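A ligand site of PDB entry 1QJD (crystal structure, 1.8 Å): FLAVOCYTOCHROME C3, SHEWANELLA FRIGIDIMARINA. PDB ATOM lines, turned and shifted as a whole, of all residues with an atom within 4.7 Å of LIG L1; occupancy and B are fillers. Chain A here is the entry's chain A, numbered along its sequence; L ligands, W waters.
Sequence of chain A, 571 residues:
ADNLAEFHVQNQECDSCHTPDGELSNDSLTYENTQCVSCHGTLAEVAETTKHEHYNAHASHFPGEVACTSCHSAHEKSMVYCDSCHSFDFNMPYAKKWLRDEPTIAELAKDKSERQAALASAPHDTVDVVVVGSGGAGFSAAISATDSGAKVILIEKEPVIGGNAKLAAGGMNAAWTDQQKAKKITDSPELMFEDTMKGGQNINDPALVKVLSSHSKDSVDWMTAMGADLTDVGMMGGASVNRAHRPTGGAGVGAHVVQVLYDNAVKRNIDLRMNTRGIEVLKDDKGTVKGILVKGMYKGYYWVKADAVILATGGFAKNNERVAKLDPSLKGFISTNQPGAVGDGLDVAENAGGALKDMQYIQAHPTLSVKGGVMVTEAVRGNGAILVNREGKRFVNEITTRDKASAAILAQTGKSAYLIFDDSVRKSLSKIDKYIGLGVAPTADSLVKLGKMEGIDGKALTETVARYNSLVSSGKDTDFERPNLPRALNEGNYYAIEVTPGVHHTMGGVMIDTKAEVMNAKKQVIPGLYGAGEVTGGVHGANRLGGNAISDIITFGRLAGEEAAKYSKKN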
ATOM      1  N   ALA A   5     -14.422 -23.590  26.827  1.00  0.00           N
ATOM      2  CA  ALA A   5     -14.759 -23.569  25.403  1.00  0.00           C
ATOM      3  C   ALA A   5     -13.532 -23.352  24.528  1.00  0.00           C
ATOM      4  O   ALA A   5     -13.329 -24.034  23.529  1.00  0.00           O
ATOM      5  CB  ALA A   5     -15.777 -22.471  25.121  1.00  0.00           C
ATOM      6  N   HIS A   8     -11.733 -26.534  24.043  1.00  0.00           N
ATOM      7  CA  HIS A   8     -12.322 -27.527  23.158  1.00  0.00           C
ATOM      8  C   HIS A   8     -12.312 -27.102  21.693  1.00  0.00           C
ATOM      9  O   HIS A   8     -12.166 -27.938  20.802  1.00  0.00           O
ATOM     10  CB  HIS A   8     -13.766 -27.826  23.559  1.00  0.00           C
ATOM     11  CG  HIS A   8     -13.899 -28.693  24.781  1.00  0.00           C
ATOM     12  ND1 HIS A   8     -13.886 -28.182  26.053  1.00  0.00           N
ATOM     13  CD2 HIS A   8     -14.082 -30.025  24.925  1.00  0.00           C
ATOM     14  CE1 HIS A   8     -14.046 -29.165  26.930  1.00  0.00           C
ATOM     15  NE2 HIS A   8     -14.154 -30.303  26.268  1.00  0.00           N
ATOM     16  N   VAL A   9     -12.498 -25.814  21.417  1.00  0.00           N
ATOM     17  CA  VAL A   9     -12.567 -25.443  19.993  1.00  0.00           C
ATOM     18  C   VAL A   9     -11.210 -25.502  19.331  1.00  0.00           C
ATOM     19  O   VAL A   9     -11.091 -25.355  18.101  1.00  0.00           O
ATOM     20  CB  VAL A   9     -13.210 -24.057  19.811  1.00  0.00           C
ATOM     21  CG1 VAL A   9     -14.549 -23.986  20.553  1.00  0.00           C
ATOM     22  CG2 VAL A   9     -12.272 -22.960  20.276  1.00  0.00           C
ATOM     23  N   CYS A  14     -18.109 -25.521  17.065  1.00  0.00           N
ATOM     24  CA  CYS A  14     -19.146 -25.059  17.986  1.00  0.00           C
ATOM     25  C   CYS A  14     -20.283 -26.044  18.147  1.00  0.00           C
ATOM     26  O   CYS A  14     -20.835 -26.183  19.252  1.00  0.00           O
ATOM     27  CB  CYS A  14     -19.701 -23.720  17.488  1.00  0.00           C
ATOM     28  SG  CYS A  14     -18.463 -22.479  17.084  1.00  0.00           S
ATOM     29  N   SER A  16     -20.183 -29.117  18.314  1.00  0.00           N
ATOM     30  CA  SER A  16     -19.920 -30.262  19.208  1.00  0.00           C
ATOM     31  C   SER A  16     -20.703 -30.094  20.500  1.00  0.00           C
ATOM     32  O   SER A  16     -21.202 -31.046  21.106  1.00  0.00           O
ATOM     33  CB  SER A  16     -18.433 -30.416  19.469  1.00  0.00           C
ATOM     34  OG  SER A  16     -17.871 -29.298  20.121  1.00  0.00           O
ATOM     35  N   CYS A  17     -20.824 -28.847  20.952  1.00  0.00           N
ATOM     36  CA  CYS A  17     -21.579 -28.580  22.187  1.00  0.00           C
ATOM     37  C   CYS A  17     -22.975 -28.047  21.931  1.00  0.00           C
ATOM     38  O   CYS A  17     -23.951 -28.391  22.615  1.00  0.00           O
ATOM     39  CB  CYS A  17     -20.770 -27.599  23.063  1.00  0.00           C
ATOM     40  SG  CYS A  17     -19.365 -28.379  23.893  1.00  0.00           S
ATOM     41  N   HIS A  18     -23.106 -27.170  20.941  1.00  0.00           N
ATOM     42  CA  HIS A  18     -24.353 -26.472  20.692  1.00  0.00           C
ATOM     43  C   HIS A  18     -25.332 -27.135  19.748  1.00  0.00           C
ATOM     44  O   HIS A  18     -25.038 -28.027  18.950  1.00  0.00           O
ATOM     45  CB  HIS A  18     -23.999 -25.091  20.088  1.00  0.00           C
ATOM     46  CG  HIS A  18     -23.402 -24.162  21.097  1.00  0.00           C
ATOM     47  ND1 HIS A  18     -24.174 -23.507  22.013  1.00  0.00           N
ATOM     48  CD2 HIS A  18     -22.129 -23.771  21.336  1.00  0.00           C
ATOM     49  CE1 HIS A  18     -23.403 -22.753  22.789  1.00  0.00           C
ATOM     50  NE2 HIS A  18     -22.155 -22.895  22.398  1.00  0.00           N
ATOM     51  N   LEU A  24     -29.080 -21.571  23.017  1.00  0.00           N
ATOM     52  CA  LEU A  24     -29.104 -22.485  24.165  1.00  0.00           C
ATOM     53  C   LEU A  24     -30.472 -23.143  24.293  1.00  0.00           C
ATOM     54  O   LEU A  24     -31.527 -22.508  24.135  1.00  0.00           O
ATOM     55  CB  LEU A  24     -28.705 -21.675  25.404  1.00  0.00           C
ATOM     56  CG  LEU A  24     -27.336 -21.022  25.322  1.00  0.00           C
ATOM     57  CD1 LEU A  24     -27.094 -20.071  26.472  1.00  0.00           C
ATOM     58  CD2 LEU A  24     -26.258 -22.100  25.258  1.00  0.00           C
ATOM     59  N   LEU A  29     -29.885 -26.143  30.466  1.00  0.00           N
ATOM     60  CA  LEU A  29     -28.841 -26.468  29.515  1.00  0.00           C
ATOM     61  C   LEU A  29     -28.854 -27.961  29.195  1.00  0.00           C
ATOM     62  O   LEU A  29     -27.838 -28.653  29.097  1.00  0.00           O
ATOM     63  CB  LEU A  29     -27.462 -25.999  30.008  1.00  0.00           C
ATOM     64  CG  LEU A  29     -27.202 -24.495  30.041  1.00  0.00           C
ATOM     65  CD1 LEU A  29     -25.780 -24.177  30.486  1.00  0.00           C
ATOM     66  CD2 LEU A  29     -27.445 -23.857  28.673  1.00  0.00           C
ATOM     67  N   GLU A  32     -26.893 -29.155  25.885  1.00  0.00           N
ATOM     68  CA  GLU A  32     -25.463 -28.902  26.011  1.00  0.00           C
ATOM     69  C   GLU A  32     -24.823 -29.906  26.965  1.00  0.00           C
ATOM     70  O   GLU A  32     -23.766 -30.464  26.640  1.00  0.00           O
ATOM     71  CB  GLU A  32     -25.280 -27.445  26.446  1.00  0.00           C
ATOM     72  CG  GLU A  32     -25.778 -26.468  25.373  1.00  0.00           C
ATOM     73  CD  GLU A  32     -27.266 -26.248  25.331  1.00  0.00           C
ATOM     74  OE1 GLU A  32     -27.988 -26.739  26.231  1.00  0.00           O
ATOM     75  OE2 GLU A  32     -27.779 -25.588  24.383  1.00  0.00           O
ATOM     76  N   THR A  69     -22.682 -28.516  33.860  1.00  0.00           N
ATOM     77  CA  THR A  69     -22.549 -27.059  33.842  1.00  0.00           C
ATOM     78  C   THR A  69     -22.775 -26.417  35.194  1.00  0.00           C
ATOM     79  O   THR A  69     -22.594 -25.198  35.291  1.00  0.00           O
ATOM     80  CB  THR A  69     -23.493 -26.396  32.814  1.00  0.00           C
ATOM     81  OG1 THR A  69     -24.812 -26.958  32.885  1.00  0.00           O
ATOM     82  CG2 THR A  69     -22.956 -26.636  31.413  1.00  0.00           C
ATOM     83  N   SER A  73     -18.505 -24.132  33.542  1.00  0.00           N
ATOM     84  CA  SER A  73     -18.990 -23.195  32.517  1.00  0.00           C
ATOM     85  C   SER A  73     -18.127 -23.296  31.274  1.00  0.00           C
ATOM     86  O   SER A  73     -17.011 -23.836  31.309  1.00  0.00           O
ATOM     87  CB  SER A  73     -19.002 -21.753  33.032  1.00  0.00           C
ATOM     88  OG  SER A  73     -19.892 -21.631  34.131  1.00  0.00           O
ATOM     89  N   ALA A  74     -18.578 -22.811  30.114  1.00  0.00           N
ATOM     90  CA  ALA A  74     -17.725 -22.987  28.940  1.00  0.00           C
ATOM     91  C   ALA A  74     -16.959 -21.733  28.576  1.00  0.00           C
ATOM     92  O   ALA A  74     -15.758 -21.769  28.337  1.00  0.00           O
ATOM     93  CB  ALA A  74     -18.558 -23.393  27.730  1.00  0.00           C
ATOM     94  N   HIS A  75     -17.666 -20.600  28.511  1.00  0.00           N
ATOM     95  CA  HIS A  75     -17.028 -19.387  27.981  1.00  0.00           C
ATOM     96  C   HIS A  75     -16.474 -18.485  29.060  1.00  0.00           C
ATOM     97  O   HIS A  75     -15.945 -17.394  28.760  1.00  0.00           O
ATOM     98  CB  HIS A  75     -18.036 -18.658  27.073  1.00  0.00           C
ATOM     99  CG  HIS A  75     -18.370 -19.492  25.874  1.00  0.00           C
ATOM    100  ND1 HIS A  75     -17.507 -19.685  24.808  1.00  0.00           N
ATOM    101  CD2 HIS A  75     -19.475 -20.216  25.590  1.00  0.00           C
ATOM    102  CE1 HIS A  75     -18.097 -20.476  23.925  1.00  0.00           C
ATOM    103  NE2 HIS A  75     -19.293 -20.821  24.372  1.00  0.00           N
ATOM    104  N   GLU A  76     -16.530 -18.900  30.326  1.00  0.00           N
ATOM    105  CA  GLU A  76     -15.930 -18.135  31.408  1.00  0.00           C
ATOM    106  C   GLU A  76     -15.412 -19.078  32.498  1.00  0.00           C
ATOM    107  O   GLU A  76     -15.831 -20.246  32.530  1.00  0.00           O
ATOM    108  CB  GLU A  76     -16.935 -17.149  31.994  1.00  0.00           C
ATOM    109  CG  GLU A  76     -18.182 -17.813  32.561  1.00  0.00           C
ATOM    110  CD  GLU A  76     -19.309 -16.853  32.839  1.00  0.00           C
ATOM    111  OE1 GLU A  76     -19.196 -16.051  33.800  1.00  0.00           O
ATOM    112  OE2 GLU A  76     -20.319 -16.886  32.103  1.00  0.00           O
ATOM    113  N   TYR A 298     -29.890 -18.285  31.683  1.00  0.00           N
ATOM    114  CA  TYR A 298     -29.270 -18.329  30.359  1.00  0.00           C
ATOM    115  C   TYR A 298     -30.177 -17.736  29.295  1.00  0.00           C
ATOM    116  O   TYR A 298     -29.697 -17.316  28.249  1.00  0.00           O
ATOM    117  CB  TYR A 298     -28.921 -19.784  30.003  1.00  0.00           C
ATOM    118  CG  TYR A 298     -27.915 -20.339  30.996  1.00  0.00           C
ATOM    119  CD1 TYR A 298     -26.597 -19.901  30.945  1.00  0.00           C
ATOM    120  CD2 TYR A 298     -28.250 -21.272  31.971  1.00  0.00           C
ATOM    121  CE1 TYR A 298     -25.630 -20.366  31.817  1.00  0.00           C
ATOM    122  CE2 TYR A 298     -27.278 -21.730  32.855  1.00  0.00           C
ATOM    123  CZ  TYR A 298     -25.975 -21.291  32.775  1.00  0.00           C
ATOM    124  OH  TYR A 298     -25.000 -21.734  33.641  1.00  0.00           O
HETATM  125 FE1  LIG L   1     -20.834 -21.844  23.512  1.00  0.00          FE
HETATM  126  C1  LIG L   1     -22.954 -20.266  25.532  1.00  0.00           C
HETATM  127  C2  LIG L   1     -21.248 -19.465  21.143  1.00  0.00           C
HETATM  128  C3  LIG L   1     -18.319 -23.228  21.542  1.00  0.00           C
HETATM  129  C4  LIG L   1     -20.723 -24.504  25.498  1.00  0.00           C
HETATM  130  N1  LIG L   1     -21.697 -20.123  23.426  1.00  0.00           N
HETATM  131  C5  LIG L   1     -22.504 -19.590  24.404  1.00  0.00           C
HETATM  132  C6  LIG L   1     -23.145 -18.372  23.959  1.00  0.00           C
HETATM  133  C7  LIG L   1     -22.727 -18.152  22.679  1.00  0.00           C
HETATM  134  C8  LIG L   1     -21.821 -19.244  22.362  1.00  0.00           C
HETATM  135  C9  LIG L   1     -22.857 -16.800  21.960  1.00  0.00           C
HETATM  136  C10 LIG L   1     -24.206 -17.604  24.745  1.00  0.00           C
HETATM  137  C11 LIG L   1     -25.624 -17.724  24.154  1.00  0.00           C
HETATM  138  C12 LIG L   1     -26.589 -16.935  25.020  1.00  0.00           C
HETATM  139  O1  LIG L   1     -27.764 -16.850  24.621  1.00  0.00           O
HETATM  140  O2  LIG L   1     -26.133 -16.420  26.059  1.00  0.00           O
HETATM  141  N2  LIG L   1     -19.903 -21.409  21.717  1.00  0.00           N
HETATM  142  C13 LIG L   1     -20.325 -20.447  20.839  1.00  0.00           C
HETATM  143  C14 LIG L   1     -19.572 -20.499  19.600  1.00  0.00           C
HETATM  144  C15 LIG L   1     -18.694 -21.529  19.717  1.00  0.00           C
HETATM  145  C16 LIG L   1     -18.928 -22.110  21.027  1.00  0.00           C
HETATM  146  C17 LIG L   1     -19.741 -19.493  18.468  1.00  0.00           C
HETATM  147  C18 LIG L   1     -17.730 -21.911  18.783  1.00  0.00           C
HETATM  148  C19 LIG L   1     -16.578 -21.067  18.495  1.00  0.00           C
HETATM  149  N3  LIG L   1     -19.704 -23.477  23.548  1.00  0.00           N
HETATM  150  C20 LIG L   1     -18.682 -23.878  22.708  1.00  0.00           C
HETATM  151  C21 LIG L   1     -18.134 -25.159  23.103  1.00  0.00           C
HETATM  152  C22 LIG L   1     -18.835 -25.559  24.198  1.00  0.00           C
HETATM  153  C23 LIG L   1     -19.807 -24.506  24.473  1.00  0.00           C
HETATM  154  C24 LIG L   1     -16.868 -25.793  22.545  1.00  0.00           C
HETATM  155  C25 LIG L   1     -18.813 -26.846  24.748  1.00  0.00           C
HETATM  156  C26 LIG L   1     -17.588 -27.350  25.353  1.00  0.00           C
HETATM  157  N4  LIG L   1     -21.695 -22.297  25.133  1.00  0.00           N
HETATM  158  C27 LIG L   1     -21.585 -23.480  25.837  1.00  0.00           C
HETATM  159  C28 LIG L   1     -22.364 -23.446  27.046  1.00  0.00           C
HETATM  160  C29 LIG L   1     -22.962 -22.224  27.107  1.00  0.00           C
HETATM  161  C30 LIG L   1     -22.510 -21.517  25.919  1.00  0.00           C
HETATM  162  C31 LIG L   1     -22.571 -24.571  28.054  1.00  0.00           C
HETATM  163  C32 LIG L   1     -23.649 -21.638  28.346  1.00  0.00           C
HETATM  164  C33 LIG L   1     -22.826 -20.537  29.050  1.00  0.00           C
HETATM  165  C34 LIG L   1     -21.442 -21.027  29.438  1.00  0.00           C
HETATM  166  O3  LIG L   1     -20.437 -20.346  29.168  1.00  0.00           O
HETATM  167  O4  LIG L   1     -21.361 -22.118  30.039  1.00  0.00           O
HETATM  168 FE1  LG2 L   2     -14.621 -32.057  27.180  1.00  0.00          FE
HETATM  169  C1  LG2 L   2     -11.289 -32.019  27.858  1.00  0.00           C
HETATM  170  C2  LG2 L   2     -15.258 -30.760  30.318  1.00  0.00           C
HETATM  171  C3  LG2 L   2     -17.744 -31.298  26.252  1.00  0.00           C
HETATM  172  C4  LG2 L   2     -14.168 -33.982  24.540  1.00  0.00           C
HETATM  173  N1  LG2 L   2     -13.518 -31.467  28.725  1.00  0.00           N
HETATM  174  C5  LG2 L   2     -12.141 -31.481  28.813  1.00  0.00           C
HETATM  175  C6  LG2 L   2     -11.710 -31.089  30.135  1.00  0.00           C
HETATM  176  C7  LG2 L   2     -12.830 -30.859  30.869  1.00  0.00           C
HETATM  177  C8  LG2 L   2     -13.956 -31.113  29.991  1.00  0.00           C
HETATM  178  C9  LG2 L   2     -12.936 -30.361  32.304  1.00  0.00           C
HETATM  179  C10 LG2 L   2     -10.271 -30.644  30.481  1.00  0.00           C
HETATM  180  C11 LG2 L   2      -9.735 -29.407  29.772  1.00  0.00           C
HETATM  181  C12 LG2 L   2      -8.319 -29.063  30.206  1.00  0.00           C
HETATM  182  O1  LG2 L   2      -7.960 -27.865  30.276  1.00  0.00           O
HETATM  183  O2  LG2 L   2      -7.558 -30.011  30.489  1.00  0.00           O
HETATM  184  N2  LG2 L   2     -16.190 -31.208  28.137  1.00  0.00           N
HETATM  185  C13 LG2 L   2     -16.329 -30.809  29.439  1.00  0.00           C
HETATM  186  C14 LG2 L   2     -17.680 -30.348  29.692  1.00  0.00           C
HETATM  187  C15 LG2 L   2     -18.349 -30.441  28.520  1.00  0.00           C
HETATM  188  C16 LG2 L   2     -17.393 -30.948  27.549  1.00  0.00           C
HETATM  189  C17 LG2 L   2     -18.275 -29.976  31.046  1.00  0.00           C
HETATM  190  C18 LG2 L   2     -19.575 -29.876  28.179  1.00  0.00           C
HETATM  191  C19 LG2 L   2     -19.933 -28.507  28.540  1.00  0.00           C
HETATM  192  N3  LG2 L   2     -15.720 -32.527  25.755  1.00  0.00           N
HETATM  193  C20 LG2 L   2     -16.941 -32.023  25.399  1.00  0.00           C
HETATM  194  C21 LG2 L   2     -17.444 -32.629  24.178  1.00  0.00           C
HETATM  195  C22 LG2 L   2     -16.497 -33.503  23.764  1.00  0.00           C
HETATM  196  C23 LG2 L   2     -15.419 -33.419  24.726  1.00  0.00           C
HETATM  197  C24 LG2 L   2     -18.790 -32.315  23.530  1.00  0.00           C
HETATM  198  C25 LG2 L   2     -16.560 -34.390  22.682  1.00  0.00           C
HETATM  199  C26 LG2 L   2     -16.917 -33.931  21.332  1.00  0.00           C
HETATM  200  N4  LG2 L   2     -13.052 -32.812  26.358  1.00  0.00           N
HETATM  201  C27 LG2 L   2     -13.045 -33.630  25.257  1.00  0.00           C
HETATM  202  C28 LG2 L   2     -11.712 -34.080  24.946  1.00  0.00           C
HETATM  203  C29 LG2 L   2     -10.889 -33.512  25.869  1.00  0.00           C
HETATM  204  C30 LG2 L   2     -11.732 -32.729  26.755  1.00  0.00           C
HETATM  205  C31 LG2 L   2     -11.327 -35.084  23.863  1.00  0.00           C
HETATM  206  C32 LG2 L   2      -9.387 -33.721  26.028  1.00  0.00           C
HETATM  207  C33 LG2 L   2      -8.965 -34.844  26.971  1.00  0.00           C
HETATM  208  C34 LG2 L   2      -9.542 -36.188  26.554  1.00  0.00           C
HETATM  209  O3  LG2 L   2      -9.056 -36.741  25.539  1.00  0.00           O
HETATM  210  O4  LG2 L   2     -10.468 -36.697  27.227  1.00  0.00           O
HETATM  211  O   HOH W   1     -24.082 -20.822  20.138  1.00  0.00           O
HETATM  212  O   HOH W   2     -29.243 -18.606  23.015  1.00  0.00           O
HETATM  213  O   HOH W   3     -20.786 -17.673  29.329  1.00  0.00           O
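NE2 of His 75 binds FE1 of LIG L1 (2.0 Å). The backbone NH (N) of His 75 is in hydrogen-bond range of an oxygen (O3) of LIG L1, at 2.9 Å. SG of Cys 14 is covalently linked to C18 of LIG L1, 1.9 Å away. SG of Cys 17 is covalently linked to C25 of LIG L1 (1.8 Å). NE2 of His 8 binds FE1 of LG2 L2 (2.0 Å). A ring nitrogen (NE2) of His 18 is bound to an iron atom (FE1) of LIG L1, at 2.0 Å. N of Ala 74 lies within hydrogen-bond range of O4 of LIG L1, at 2.9 Å.
Water W3 lies within hydrogen-bond range of an oxygen (O3) of LIG L1 (2.7 Å) and the side-chain carboxylate (OE2) of Glu 76 (2.9 Å). Water W2 lies within hydrogen-bond range of O1 of LIG L1 and N of Leu 24.
CB of His 8 touches C24 of LIG L1, 3.8 Å away. Val 9 touches LIG L1. CD1 of Leu 24 touches C12 of LIG L1 (3.5 Å). Leu 29 touches LIG L1 (CD1 to C32, 3.9 Å). Thr 69 touches LIG L1 (CG2 to C31, 3.96 Å). CA of Ser 73 touches O4 of LIG L1, at 3.6 Å. Tyr 298 touches LIG L1 (CE1 to C33, 3.9 Å). Within 4 Å of LIG L1: His 8, Val 9, Cys 14, Cys 17, His 18, Leu 24, Leu 29, Thr 69, Ser 73, Ala 74, His 75 and Tyr 298.
O of Ala 74 sits at hydrogen-bond distance from N of Ala 5.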
